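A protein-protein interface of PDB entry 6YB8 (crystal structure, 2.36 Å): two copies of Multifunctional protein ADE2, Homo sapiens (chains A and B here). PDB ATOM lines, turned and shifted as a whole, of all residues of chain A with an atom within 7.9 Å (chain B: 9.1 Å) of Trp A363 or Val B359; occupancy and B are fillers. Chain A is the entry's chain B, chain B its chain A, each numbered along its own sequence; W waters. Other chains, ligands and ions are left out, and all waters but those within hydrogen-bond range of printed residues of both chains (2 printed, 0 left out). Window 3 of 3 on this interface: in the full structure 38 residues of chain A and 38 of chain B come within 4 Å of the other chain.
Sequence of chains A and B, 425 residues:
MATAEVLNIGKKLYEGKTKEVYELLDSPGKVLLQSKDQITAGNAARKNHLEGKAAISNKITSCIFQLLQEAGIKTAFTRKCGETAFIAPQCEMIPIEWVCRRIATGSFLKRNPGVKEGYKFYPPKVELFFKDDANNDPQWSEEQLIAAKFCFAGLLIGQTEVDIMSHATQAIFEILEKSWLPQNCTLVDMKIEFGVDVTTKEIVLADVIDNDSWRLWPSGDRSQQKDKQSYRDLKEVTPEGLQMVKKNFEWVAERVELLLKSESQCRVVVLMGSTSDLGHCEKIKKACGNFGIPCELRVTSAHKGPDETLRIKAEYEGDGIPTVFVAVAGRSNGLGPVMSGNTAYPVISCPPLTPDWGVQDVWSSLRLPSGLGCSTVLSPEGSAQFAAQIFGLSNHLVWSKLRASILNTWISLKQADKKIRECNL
The backbone carbonyl oxygen (O) of Thr A376 is in hydrogen-bond range of the backbone NH (N) of Thr B376, 2.9 Å away.
The backbone carbonyl oxygen (O) of Ser A365 lies within hydrogen-bond range of the side-chain hydroxyl (OG1) of Thr A376.
CA of Val A359 touches CZ2 of Trp B363, at 3.98 Å.
Val A362 touches Trp B363 (CG1 to CZ2, 3.7 Å).
CA of Val B359 touches CZ2 of Trp A363, 3.998 Å away.
CH2 of Trp A363 touches CG1 of Val B362, 3.8 Å away.
Leu A366 touches Leu B366.
Leu B378 touches Leu A366.
Printed residues of chain B within 4 Å of Val A359: Trp B363 (3.98 Å).
Asp A361 touches none of the printed residues of chain B.
Val A362 touches just one residue of chain B: Trp B363 (3.7 Å).
No residue of chain B comes within 4 Å of Ser A364.
Gly B358 touches none of the printed residues of chain A.
Of the printed residues of chain A, Val B359 touches Trp A363.
Printed residues of chain A within 4 Å of Thr B376: Thr A376.
Printed residues of chain A within 4 Å of Leu B378: Leu A366.
The nearest printed residue of chain A that does not touch Val B359 is Val A359 (6.6 Å).
Hydrophobic or aromatic side chains of chain A within 4 Å of the printed part of chain B: Val A362, Trp A363 and Leu A366.
Of the 17 printed residues of chain B, 6 touch a printed residue of chain A.
Hydrophobic or aromatic side chains of chain B that line the printed part of chain A: Val B362, Trp B363, Leu B366 and Leu B378.
Val A359 touches Trp B363, and with the chains exchanged Trp A363 touches Val B359.
Val A362 touches Trp B363, and with the chains exchanged Trp A363 touches Val B362.
Leu B366 touches its own counterpart, Leu A366.
Thr A376 touches its own counterpart, Thr B376.
Positions printed for both chains: 331, 351, 353, 357, 358, 359, 360, 361, 362, 363, 364, 366 and 376.
Water W1 bridges O of Leu A366 (2.6 Å) and N of Leu B378 (3.3 Å).
Water W2 lies within hydrogen-bond range of OG1 of Thr A376 (2.7 Å), O of Ser A365 (3.2 Å) and O of Thr B376 (3.4 Å).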
ATOM      1  N   ARG A 331      22.916  -7.887 -13.765  1.00  0.00           N
ATOM      2  CA  ARG A 331      22.926  -6.609 -14.519  1.00  0.00           C
ATOM      3  C   ARG A 331      23.129  -6.938 -16.012  1.00  0.00           C
ATOM      4  O   ARG A 331      22.452  -7.881 -16.486  1.00  0.00           O
ATOM      5  CB  ARG A 331      23.995  -5.703 -13.879  1.00  0.00           C
ATOM      6  CG  ARG A 331      23.849  -5.578 -12.368  1.00  0.00           C
ATOM      7  CD  ARG A 331      24.554  -4.388 -11.777  1.00  0.00           C
ATOM      8  NE  ARG A 331      24.459  -4.452 -10.322  1.00  0.00           N
ATOM      9  CZ  ARG A 331      25.232  -3.789  -9.457  1.00  0.00           C
ATOM     10  NH1 ARG A 331      26.176  -2.961  -9.892  1.00  0.00           N
ATOM     11  NH2 ARG A 331      25.053  -3.984  -8.153  1.00  0.00           N
ATOM     12  N   SER A 332      23.987  -6.199 -16.730  1.00  0.00           N
ATOM     13  CA  SER A 332      24.275  -6.402 -18.180  1.00  0.00           C
ATOM     14  C   SER A 332      25.250  -7.577 -18.305  1.00  0.00           C
ATOM     15  O   SER A 332      26.466  -7.417 -18.032  1.00  0.00           O
ATOM     16  CB  SER A 332      24.783  -5.143 -18.844  1.00  0.00           C
ATOM     17  OG  SER A 332      25.341  -5.374 -20.137  1.00  0.00           O
ATOM     18  N   ASN A 333      24.683  -8.733 -18.618  1.00  0.00           N
ATOM     19  CA  ASN A 333      25.413 -10.005 -18.817  1.00  0.00           C
ATOM     20  C   ASN A 333      26.226  -9.851 -20.118  1.00  0.00           C
ATOM     21  O   ASN A 333      25.600  -9.826 -21.216  1.00  0.00           O
ATOM     22  CB  ASN A 333      24.435 -11.192 -18.738  1.00  0.00           C
ATOM     23  CG  ASN A 333      25.028 -12.509 -19.213  1.00  0.00           C
ATOM     24  OD1 ASN A 333      26.231 -12.598 -19.415  1.00  0.00           O
ATOM     25  ND2 ASN A 333      24.206 -13.533 -19.383  1.00  0.00           N
ATOM     26  N   PRO A 351      21.227 -16.051 -15.451  1.00  0.00           N
ATOM     27  CA  PRO A 351      21.483 -14.823 -14.702  1.00  0.00           C
ATOM     28  C   PRO A 351      20.746 -14.896 -13.379  1.00  0.00           C
ATOM     29  O   PRO A 351      19.595 -15.346 -13.383  1.00  0.00           O
ATOM     30  CB  PRO A 351      20.896 -13.710 -15.590  1.00  0.00           C
ATOM     31  CG  PRO A 351      19.819 -14.408 -16.400  1.00  0.00           C
ATOM     32  CD  PRO A 351      20.331 -15.818 -16.607  1.00  0.00           C
ATOM     33  N   LEU A 353      18.580 -13.373 -11.617  1.00  0.00           N
ATOM     34  CA  LEU A 353      17.494 -12.350 -11.701  1.00  0.00           C
ATOM     35  C   LEU A 353      16.775 -12.295 -10.361  1.00  0.00           C
ATOM     36  O   LEU A 353      16.632 -13.349  -9.722  1.00  0.00           O
ATOM     37  CB  LEU A 353      16.493 -12.664 -12.829  1.00  0.00           C
ATOM     38  CG  LEU A 353      17.056 -12.605 -14.257  1.00  0.00           C
ATOM     39  CD1 LEU A 353      15.954 -12.754 -15.299  1.00  0.00           C
ATOM     40  CD2 LEU A 353      17.857 -11.332 -14.509  1.00  0.00           C
ATOM     41  N   TRP A 357      14.950  -5.648 -10.775  1.00  0.00           N
ATOM     42  CA  TRP A 357      15.474  -5.187 -12.093  1.00  0.00           C
ATOM     43  C   TRP A 357      15.564  -6.340 -13.116  1.00  0.00           C
ATOM     44  O   TRP A 357      16.061  -6.098 -14.260  1.00  0.00           O
ATOM     45  CB  TRP A 357      16.840  -4.541 -11.873  1.00  0.00           C
ATOM     46  CG  TRP A 357      16.851  -3.332 -10.990  1.00  0.00           C
ATOM     47  CD1 TRP A 357      17.403  -3.248  -9.742  1.00  0.00           C
ATOM     48  CD2 TRP A 357      16.370  -2.012 -11.311  1.00  0.00           C
ATOM     49  NE1 TRP A 357      17.298  -1.967  -9.259  1.00  0.00           N
ATOM     50  CE2 TRP A 357      16.667  -1.183 -10.193  1.00  0.00           C
ATOM     51  CE3 TRP A 357      15.746  -1.431 -12.431  1.00  0.00           C
ATOM     52  CZ2 TRP A 357      16.330   0.175 -10.156  1.00  0.00           C
ATOM     53  CZ3 TRP A 357      15.416  -0.084 -12.394  1.00  0.00           C
ATOM     54  CH2 TRP A 357      15.713   0.706 -11.276  1.00  0.00           C
ATOM     55  N   GLY A 358      15.105  -7.538 -12.739  1.00  0.00           N
ATOM     56  CA  GLY A 358      15.161  -8.767 -13.547  1.00  0.00           C
ATOM     57  C   GLY A 358      14.419  -8.656 -14.869  1.00  0.00           C
ATOM     58  O   GLY A 358      14.965  -9.229 -15.859  1.00  0.00           O
ATOM     59  N   VAL A 359      13.255  -7.973 -14.912  1.00  0.00           N
ATOM     60  CA  VAL A 359      12.501  -7.725 -16.185  1.00  0.00           C
ATOM     61  C   VAL A 359      13.430  -7.007 -17.189  1.00  0.00           C
ATOM     62  O   VAL A 359      13.323  -7.295 -18.402  1.00  0.00           O
ATOM     63  CB  VAL A 359      11.187  -6.935 -15.982  1.00  0.00           C
ATOM     64  CG1 VAL A 359      10.607  -6.467 -17.323  1.00  0.00           C
ATOM     65  CG2 VAL A 359      10.144  -7.719 -15.180  1.00  0.00           C
ATOM     66  N   GLN A 360      14.299  -6.102 -16.721  1.00  0.00           N
ATOM     67  CA  GLN A 360      15.185  -5.264 -17.576  1.00  0.00           C
ATOM     68  C   GLN A 360      16.474  -6.050 -17.872  1.00  0.00           C
ATOM     69  O   GLN A 360      16.919  -6.051 -19.052  1.00  0.00           O
ATOM     70  CB  GLN A 360      15.529  -3.932 -16.885  1.00  0.00           C
ATOM     71  CG  GLN A 360      14.391  -2.925 -16.733  1.00  0.00           C
ATOM     72  CD  GLN A 360      13.305  -3.331 -15.762  1.00  0.00           C
ATOM     73  OE1 GLN A 360      13.539  -3.659 -14.594  1.00  0.00           O
ATOM     74  NE2 GLN A 360      12.082  -3.286 -16.260  1.00  0.00           N
ATOM     75  N   ASP A 361      17.028  -6.728 -16.856  1.00  0.00           N
ATOM     76  CA  ASP A 361      18.346  -7.408 -16.969  1.00  0.00           C
ATOM     77  C   ASP A 361      18.307  -8.596 -17.939  1.00  0.00           C
ATOM     78  O   ASP A 361      19.279  -8.749 -18.670  1.00  0.00           O
ATOM     79  CB  ASP A 361      18.894  -7.794 -15.595  1.00  0.00           C
ATOM     80  CG  ASP A 361      19.380  -6.589 -14.808  1.00  0.00           C
ATOM     81  OD1 ASP A 361      19.839  -5.565 -15.455  1.00  0.00           O
ATOM     82  OD2 ASP A 361      19.299  -6.680 -13.568  1.00  0.00           O
ATOM     83  N   VAL A 362      17.229  -9.371 -17.979  1.00  0.00           N
ATOM     84  CA  VAL A 362      17.085 -10.619 -18.804  1.00  0.00           C
ATOM     85  C   VAL A 362      17.423 -10.326 -20.286  1.00  0.00           C
ATOM     86  O   VAL A 362      17.940 -11.241 -20.985  1.00  0.00           O
ATOM     87  CB  VAL A 362      15.661 -11.221 -18.663  1.00  0.00           C
ATOM     88  CG1 VAL A 362      14.612 -10.387 -19.396  1.00  0.00           C
ATOM     89  CG2 VAL A 362      15.599 -12.678 -19.102  1.00  0.00           C
ATOM     90  N   TRP A 363      17.099  -9.127 -20.783  1.00  0.00           N
ATOM     91  CA  TRP A 363      17.194  -8.838 -22.240  1.00  0.00           C
ATOM     92  C   TRP A 363      18.665  -8.859 -22.695  1.00  0.00           C
ATOM     93  O   TRP A 363      18.888  -9.186 -23.897  1.00  0.00           O
ATOM     94  CB  TRP A 363      16.419  -7.563 -22.611  1.00  0.00           C
ATOM     95  CG  TRP A 363      14.931  -7.789 -22.561  1.00  0.00           C
ATOM     96  CD1 TRP A 363      14.067  -7.411 -21.569  1.00  0.00           C
ATOM     97  CD2 TRP A 363      14.124  -8.471 -23.543  1.00  0.00           C
ATOM     98  NE1 TRP A 363      12.786  -7.808 -21.863  1.00  0.00           N
ATOM     99  CE2 TRP A 363      12.782  -8.462 -23.062  1.00  0.00           C
ATOM    100  CE3 TRP A 363      14.382  -9.029 -24.803  1.00  0.00           C
ATOM    101  CZ2 TRP A 363      11.718  -9.025 -23.779  1.00  0.00           C
ATOM    102  CZ3 TRP A 363      13.332  -9.598 -25.504  1.00  0.00           C
ATOM    103  CH2 TRP A 363      12.021  -9.600 -25.001  1.00  0.00           C
ATOM    104  N   SER A 364      19.620  -8.633 -21.770  1.00  0.00           N
ATOM    105  CA  SER A 364      21.086  -8.701 -22.034  1.00  0.00           C
ATOM    106  C   SER A 364      21.532 -10.136 -22.363  1.00  0.00           C
ATOM    107  O   SER A 364      22.568 -10.283 -23.061  1.00  0.00           O
ATOM    108  CB  SER A 364      21.911  -8.088 -20.906  1.00  0.00           C
ATOM    109  OG  SER A 364      22.012  -8.939 -19.780  1.00  0.00           O
ATOM    110  N   SER A 365      20.809 -11.157 -21.876  1.00  0.00           N
ATOM    111  CA  SER A 365      21.061 -12.603 -22.155  1.00  0.00           C
ATOM    112  C   SER A 365      20.367 -13.044 -23.464  1.00  0.00           C
ATOM    113  O   SER A 365      20.935 -13.957 -24.151  1.00  0.00           O
ATOM    114  CB  SER A 365      20.642 -13.469 -20.986  1.00  0.00           C
ATOM    115  OG  SER A 365      21.383 -13.171 -19.810  1.00  0.00           O
ATOM    116  N   LEU A 366      19.252 -12.390 -23.844  1.00  0.00           N
ATOM    117  CA  LEU A 366      18.257 -12.897 -24.849  1.00  0.00           C
ATOM    118  C   LEU A 366      18.519 -12.358 -26.267  1.00  0.00           C
ATOM    119  O   LEU A 366      18.381 -13.132 -27.242  1.00  0.00           O
ATOM    120  CB  LEU A 366      16.848 -12.485 -24.415  1.00  0.00           C
ATOM    121  CG  LEU A 366      16.271 -13.211 -23.198  1.00  0.00           C
ATOM    122  CD1 LEU A 366      14.939 -12.587 -22.796  1.00  0.00           C
ATOM    123  CD2 LEU A 366      16.121 -14.707 -23.454  1.00  0.00           C
ATOM    124  N   ARG A 367      18.852 -11.073 -26.382  1.00  0.00           N
ATOM    125  CA  ARG A 367      18.932 -10.356 -27.679  1.00  0.00           C
ATOM    126  C   ARG A 367      20.415 -10.226 -28.021  1.00  0.00           C
ATOM    127  O   ARG A 367      21.033  -9.226 -27.600  1.00  0.00           O
ATOM    128  CB  ARG A 367      18.168  -9.022 -27.614  1.00  0.00           C
ATOM    129  CG  ARG A 367      16.708  -9.125 -28.065  1.00  0.00           C
ATOM    130  CD  ARG A 367      15.973  -7.785 -28.090  1.00  0.00           C
ATOM    131  NE  ARG A 367      16.636  -6.824 -28.976  1.00  0.00           N
ATOM    132  CZ  ARG A 367      16.531  -6.787 -30.310  1.00  0.00           C
ATOM    133  NH1 ARG A 367      15.763  -7.664 -30.941  1.00  0.00           N
ATOM    134  NH2 ARG A 367      17.193  -5.875 -31.013  1.00  0.00           N
ATOM    135  N   LEU A 368      20.957 -11.223 -28.724  1.00  0.00           N
ATOM    136  CA  LEU A 368      22.413 -11.332 -29.026  1.00  0.00           C
ATOM    137  C   LEU A 368      22.657 -11.063 -30.516  1.00  0.00           C
ATOM    138  O   LEU A 368      21.811 -11.386 -31.362  1.00  0.00           O
ATOM    139  CB  LEU A 368      22.913 -12.714 -28.583  1.00  0.00           C
ATOM    140  CG  LEU A 368      22.598 -13.093 -27.129  1.00  0.00           C
ATOM    141  CD1 LEU A 368      23.199 -14.438 -26.752  1.00  0.00           C
ATOM    142  CD2 LEU A 368      23.075 -12.021 -26.158  1.00  0.00           C
ATOM    143  N   THR A 376      19.416 -19.282 -22.835  1.00  0.00           N
ATOM    144  CA  THR A 376      19.009 -18.712 -21.539  1.00  0.00           C
ATOM    145  C   THR A 376      18.128 -19.741 -20.847  1.00  0.00           C
ATOM    146  O   THR A 376      17.237 -20.307 -21.503  1.00  0.00           O
ATOM    147  CB  THR A 376      18.354 -17.343 -21.748  1.00  0.00           C
ATOM    148  OG1 THR A 376      19.323 -16.546 -22.448  1.00  0.00           O
ATOM    149  CG2 THR A 376      17.904 -16.676 -20.463  1.00  0.00           C
ATOM    150  N   ARG B 331       2.754 -16.615 -29.503  1.00  0.00           N
ATOM    151  CA  ARG B 331       1.795 -16.295 -28.423  1.00  0.00           C
ATOM    152  C   ARG B 331       2.258 -17.052 -27.163  1.00  0.00           C
ATOM    153  O   ARG B 331       3.493 -17.031 -26.893  1.00  0.00           O
ATOM    154  CB  ARG B 331       0.388 -16.623 -28.940  1.00  0.00           C
ATOM    155  CG  ARG B 331       0.074 -16.028 -30.314  1.00  0.00           C
ATOM    156  CD  ARG B 331      -1.395 -15.732 -30.520  1.00  0.00           C
ATOM    157  NE  ARG B 331      -1.658 -15.313 -31.885  1.00  0.00           N
ATOM    158  CZ  ARG B 331      -2.833 -15.436 -32.520  1.00  0.00           C
ATOM    159  NH1 ARG B 331      -3.894 -15.960 -31.911  1.00  0.00           N
ATOM    160  NH2 ARG B 331      -2.926 -15.031 -33.780  1.00  0.00           N
ATOM    161  N   PRO B 351      10.745 -19.103 -30.162  1.00  0.00           N
ATOM    162  CA  PRO B 351       9.454 -18.521 -30.524  1.00  0.00           C
ATOM    163  C   PRO B 351       9.662 -17.507 -31.633  1.00  0.00           C
ATOM    164  O   PRO B 351      10.638 -16.737 -31.565  1.00  0.00           O
ATOM    165  CB  PRO B 351       8.963 -17.795 -29.266  1.00  0.00           C
ATOM    166  CG  PRO B 351      10.260 -17.471 -28.522  1.00  0.00           C
ATOM    167  CD  PRO B 351      11.208 -18.617 -28.846  1.00  0.00           C
ATOM    168  N   LEU B 353       9.025 -14.489 -32.345  1.00  0.00           N
ATOM    169  CA  LEU B 353       8.706 -13.167 -31.758  1.00  0.00           C
ATOM    170  C   LEU B 353       8.722 -12.127 -32.876  1.00  0.00           C
ATOM    171  O   LEU B 353       9.539 -12.272 -33.812  1.00  0.00           O
ATOM    172  CB  LEU B 353       9.735 -12.789 -30.684  1.00  0.00           C
ATOM    173  CG  LEU B 353       9.774 -13.646 -29.415  1.00  0.00           C
ATOM    174  CD1 LEU B 353      10.630 -12.940 -28.345  1.00  0.00           C
ATOM    175  CD2 LEU B 353       8.368 -13.983 -28.888  1.00  0.00           C
ATOM    176  N   THR B 354       7.844 -11.139 -32.766  1.00  0.00           N
ATOM    177  CA  THR B 354       7.823  -9.909 -33.607  1.00  0.00           C
ATOM    178  C   THR B 354       7.702  -8.725 -32.636  1.00  0.00           C
ATOM    179  O   THR B 354       7.273  -8.897 -31.494  1.00  0.00           O
ATOM    180  CB  THR B 354       6.738  -9.988 -34.707  1.00  0.00           C
ATOM    181  OG1 THR B 354       5.536  -9.407 -34.192  1.00  0.00           O
ATOM    182  CG2 THR B 354       6.459 -11.399 -35.206  1.00  0.00           C
ATOM    183  N   PRO B 355       8.076  -7.482 -33.024  1.00  0.00           N
ATOM    184  CA  PRO B 355       7.951  -6.333 -32.110  1.00  0.00           C
ATOM    185  C   PRO B 355       6.517  -5.965 -31.654  1.00  0.00           C
ATOM    186  O   PRO B 355       6.369  -5.171 -30.755  1.00  0.00           O
ATOM    187  CB  PRO B 355       8.582  -5.173 -32.908  1.00  0.00           C
ATOM    188  CG  PRO B 355       9.453  -5.876 -33.959  1.00  0.00           C
ATOM    189  CD  PRO B 355       8.678  -7.126 -34.323  1.00  0.00           C
ATOM    190  N   ASP B 356       5.471  -6.544 -32.251  1.00  0.00           N
ATOM    191  CA  ASP B 356       4.060  -6.236 -31.867  1.00  0.00           C
ATOM    192  C   ASP B 356       3.825  -6.676 -30.401  1.00  0.00           C
ATOM    193  O   ASP B 356       3.342  -5.856 -29.573  1.00  0.00           O
ATOM    194  CB  ASP B 356       3.065  -6.837 -32.876  1.00  0.00           C
ATOM    195  CG  ASP B 356       2.907  -6.059 -34.195  1.00  0.00           C
ATOM    196  OD1 ASP B 356       3.305  -4.856 -34.284  1.00  0.00           O
ATOM    197  OD2 ASP B 356       2.371  -6.656 -35.154  1.00  0.00           O
ATOM    198  N   TRP B 357       4.092  -7.952 -30.097  1.00  0.00           N
ATOM    199  CA  TRP B 357       3.708  -8.628 -28.828  1.00  0.00           C
ATOM    200  C   TRP B 357       4.864  -9.473 -28.266  1.00  0.00           C
ATOM    201  O   TRP B 357       4.650 -10.149 -27.226  1.00  0.00           O
ATOM    202  CB  TRP B 357       2.457  -9.474 -29.072  1.00  0.00           C
ATOM    203  CG  TRP B 357       1.255  -8.710 -29.543  1.00  0.00           C
ATOM    204  CD1 TRP B 357       0.699  -8.747 -30.797  1.00  0.00           C
ATOM    205  CD2 TRP B 357       0.412  -7.841 -28.754  1.00  0.00           C
ATOM    206  NE1 TRP B 357      -0.421  -7.952 -30.844  1.00  0.00           N
ATOM    207  CE2 TRP B 357      -0.641  -7.410 -29.601  1.00  0.00           C
ATOM    208  CE3 TRP B 357       0.414  -7.430 -27.412  1.00  0.00           C
ATOM    209  CZ2 TRP B 357      -1.666  -6.572 -29.152  1.00  0.00           C
ATOM    210  CZ3 TRP B 357      -0.610  -6.610 -26.966  1.00  0.00           C
ATOM    211  CH2 TRP B 357      -1.621  -6.171 -27.831  1.00  0.00           C
ATOM    212  N   GLY B 358       6.035  -9.451 -28.913  1.00  0.00           N
ATOM    213  CA  GLY B 358       7.239 -10.226 -28.532  1.00  0.00           C
ATOM    214  C   GLY B 358       7.678 -10.024 -27.081  1.00  0.00           C
ATOM    215  O   GLY B 358       7.956 -11.054 -26.410  1.00  0.00           O
ATOM    216  N   VAL B 359       7.694  -8.772 -26.603  1.00  0.00           N
ATOM    217  CA  VAL B 359       8.027  -8.402 -25.184  1.00  0.00           C
ATOM    218  C   VAL B 359       7.100  -9.157 -24.206  1.00  0.00           C
ATOM    219  O   VAL B 359       7.553  -9.496 -23.114  1.00  0.00           O
ATOM    220  CB  VAL B 359       7.962  -6.881 -24.923  1.00  0.00           C
ATOM    221  CG1 VAL B 359       8.291  -6.581 -23.465  1.00  0.00           C
ATOM    222  CG2 VAL B 359       8.855  -6.066 -25.869  1.00  0.00           C
ATOM    223  N   GLN B 360       5.856  -9.438 -24.586  1.00  0.00           N
ATOM    224  CA  GLN B 360       4.843 -10.139 -23.739  1.00  0.00           C
ATOM    225  C   GLN B 360       4.967 -11.663 -23.935  1.00  0.00           C
ATOM    226  O   GLN B 360       4.976 -12.439 -22.912  1.00  0.00           O
ATOM    227  CB  GLN B 360       3.427  -9.629 -24.065  1.00  0.00           C
ATOM    228  CG  GLN B 360       3.153  -8.168 -23.657  1.00  0.00           C
ATOM    229  CD  GLN B 360       3.831  -7.087 -24.478  1.00  0.00           C
ATOM    230  OE1 GLN B 360       3.853  -7.091 -25.703  1.00  0.00           O
ATOM    231  NE2 GLN B 360       4.400  -6.114 -23.802  1.00  0.00           N
ATOM    232  N   ASP B 361       5.121 -12.088 -25.191  1.00  0.00           N
ATOM    233  CA  ASP B 361       5.059 -13.528 -25.573  1.00  0.00           C
ATOM    234  C   ASP B 361       6.243 -14.343 -25.018  1.00  0.00           C
ATOM    235  O   ASP B 361       6.001 -15.509 -24.706  1.00  0.00           O
ATOM    236  CB  ASP B 361       4.912 -13.669 -27.091  1.00  0.00           C
ATOM    237  CG  ASP B 361       3.518 -13.287 -27.586  1.00  0.00           C
ATOM    238  OD1 ASP B 361       2.518 -13.426 -26.796  1.00  0.00           O
ATOM    239  OD2 ASP B 361       3.441 -12.817 -28.741  1.00  0.00           O
ATOM    240  N   VAL B 362       7.447 -13.752 -24.921  1.00  0.00           N
ATOM    241  CA  VAL B 362       8.746 -14.420 -24.581  1.00  0.00           C
ATOM    242  C   VAL B 362       8.695 -15.008 -23.153  1.00  0.00           C
ATOM    243  O   VAL B 362       9.347 -16.049 -22.901  1.00  0.00           O
ATOM    244  CB  VAL B 362       9.933 -13.436 -24.716  1.00  0.00           C
ATOM    245  CG1 VAL B 362       9.971 -12.424 -23.544  1.00  0.00           C
ATOM    246  CG2 VAL B 362      11.266 -14.169 -24.844  1.00  0.00           C
ATOM    247  N   TRP B 363       7.997 -14.353 -22.227  1.00  0.00           N
ATOM    248  CA  TRP B 363       7.945 -14.788 -20.802  1.00  0.00           C
ATOM    249  C   TRP B 363       7.287 -16.186 -20.661  1.00  0.00           C
ATOM    250  O   TRP B 363       7.651 -16.891 -19.710  1.00  0.00           O
ATOM    251  CB  TRP B 363       7.285 -13.690 -19.939  1.00  0.00           C
ATOM    252  CG  TRP B 363       8.183 -12.495 -19.777  1.00  0.00           C
ATOM    253  CD1 TRP B 363       8.123 -11.302 -20.455  1.00  0.00           C
ATOM    254  CD2 TRP B 363       9.331 -12.392 -18.909  1.00  0.00           C
ATOM    255  NE1 TRP B 363       9.151 -10.469 -20.081  1.00  0.00           N
ATOM    256  CE2 TRP B 363       9.898 -11.103 -19.117  1.00  0.00           C
ATOM    257  CE3 TRP B 363       9.923 -13.251 -17.978  1.00  0.00           C
ATOM    258  CZ2 TRP B 363      11.030 -10.667 -18.422  1.00  0.00           C
ATOM    259  CZ3 TRP B 363      11.031 -12.808 -17.287  1.00  0.00           C
ATOM    260  CH2 TRP B 363      11.572 -11.537 -17.500  1.00  0.00           C
ATOM    261  N   SER B 364       6.422 -16.594 -21.596  1.00  0.00           N
ATOM    262  CA  SER B 364       5.810 -17.954 -21.672  1.00  0.00           C
ATOM    263  C   SER B 364       6.871 -19.043 -21.944  1.00  0.00           C
ATOM    264  O   SER B 364       6.614 -20.196 -21.579  1.00  0.00           O
ATOM    265  CB  SER B 364       4.673 -18.027 -22.708  1.00  0.00           C
ATOM    266  OG  SER B 364       5.151 -17.947 -24.070  1.00  0.00           O
ATOM    267  N   LEU B 366      10.187 -18.525 -20.831  1.00  0.00           N
ATOM    268  CA  LEU B 366      11.295 -18.219 -19.874  1.00  0.00           C
ATOM    269  C   LEU B 366      10.978 -18.624 -18.425  1.00  0.00           C
ATOM    270  O   LEU B 366      11.884 -19.158 -17.740  1.00  0.00           O
ATOM    271  CB  LEU B 366      11.585 -16.721 -19.908  1.00  0.00           C
ATOM    272  CG  LEU B 366      12.286 -16.194 -21.148  1.00  0.00           C
ATOM    273  CD1 LEU B 366      12.332 -14.660 -21.073  1.00  0.00           C
ATOM    274  CD2 LEU B 366      13.676 -16.815 -21.286  1.00  0.00           C
ATOM    275  N   THR B 376      15.788 -21.129 -23.936  1.00  0.00           N
ATOM    276  CA  THR B 376      15.255 -20.194 -24.947  1.00  0.00           C
ATOM    277  C   THR B 376      16.408 -19.590 -25.737  1.00  0.00           C
ATOM    278  O   THR B 376      17.416 -19.195 -25.125  1.00  0.00           O
ATOM    279  CB  THR B 376      14.318 -19.157 -24.330  1.00  0.00           C
ATOM    280  OG1 THR B 376      13.462 -19.886 -23.451  1.00  0.00           O
ATOM    281  CG2 THR B 376      13.516 -18.425 -25.386  1.00  0.00           C
ATOM    282  N   LEU B 378      16.303 -16.981 -29.116  1.00  0.00           N
ATOM    283  CA  LEU B 378      15.404 -16.178 -29.991  1.00  0.00           C
ATOM    284  C   LEU B 378      15.856 -16.296 -31.452  1.00  0.00           C
ATOM    285  O   LEU B 378      14.996 -16.461 -32.326  1.00  0.00           O
ATOM    286  CB  LEU B 378      15.333 -14.734 -29.490  1.00  0.00           C
ATOM    287  CG  LEU B 378      14.918 -14.626 -28.023  1.00  0.00           C
ATOM    288  CD1 LEU B 378      14.700 -13.181 -27.626  1.00  0.00           C
ATOM    289  CD2 LEU B 378      13.661 -15.442 -27.745  1.00  0.00           C
HETATM  290  O   HOH W   1      18.550 -15.731 -27.068  1.00  0.00           O
HETATM  291  O   HOH W   2      19.854 -16.858 -25.100  1.00  0.00           O
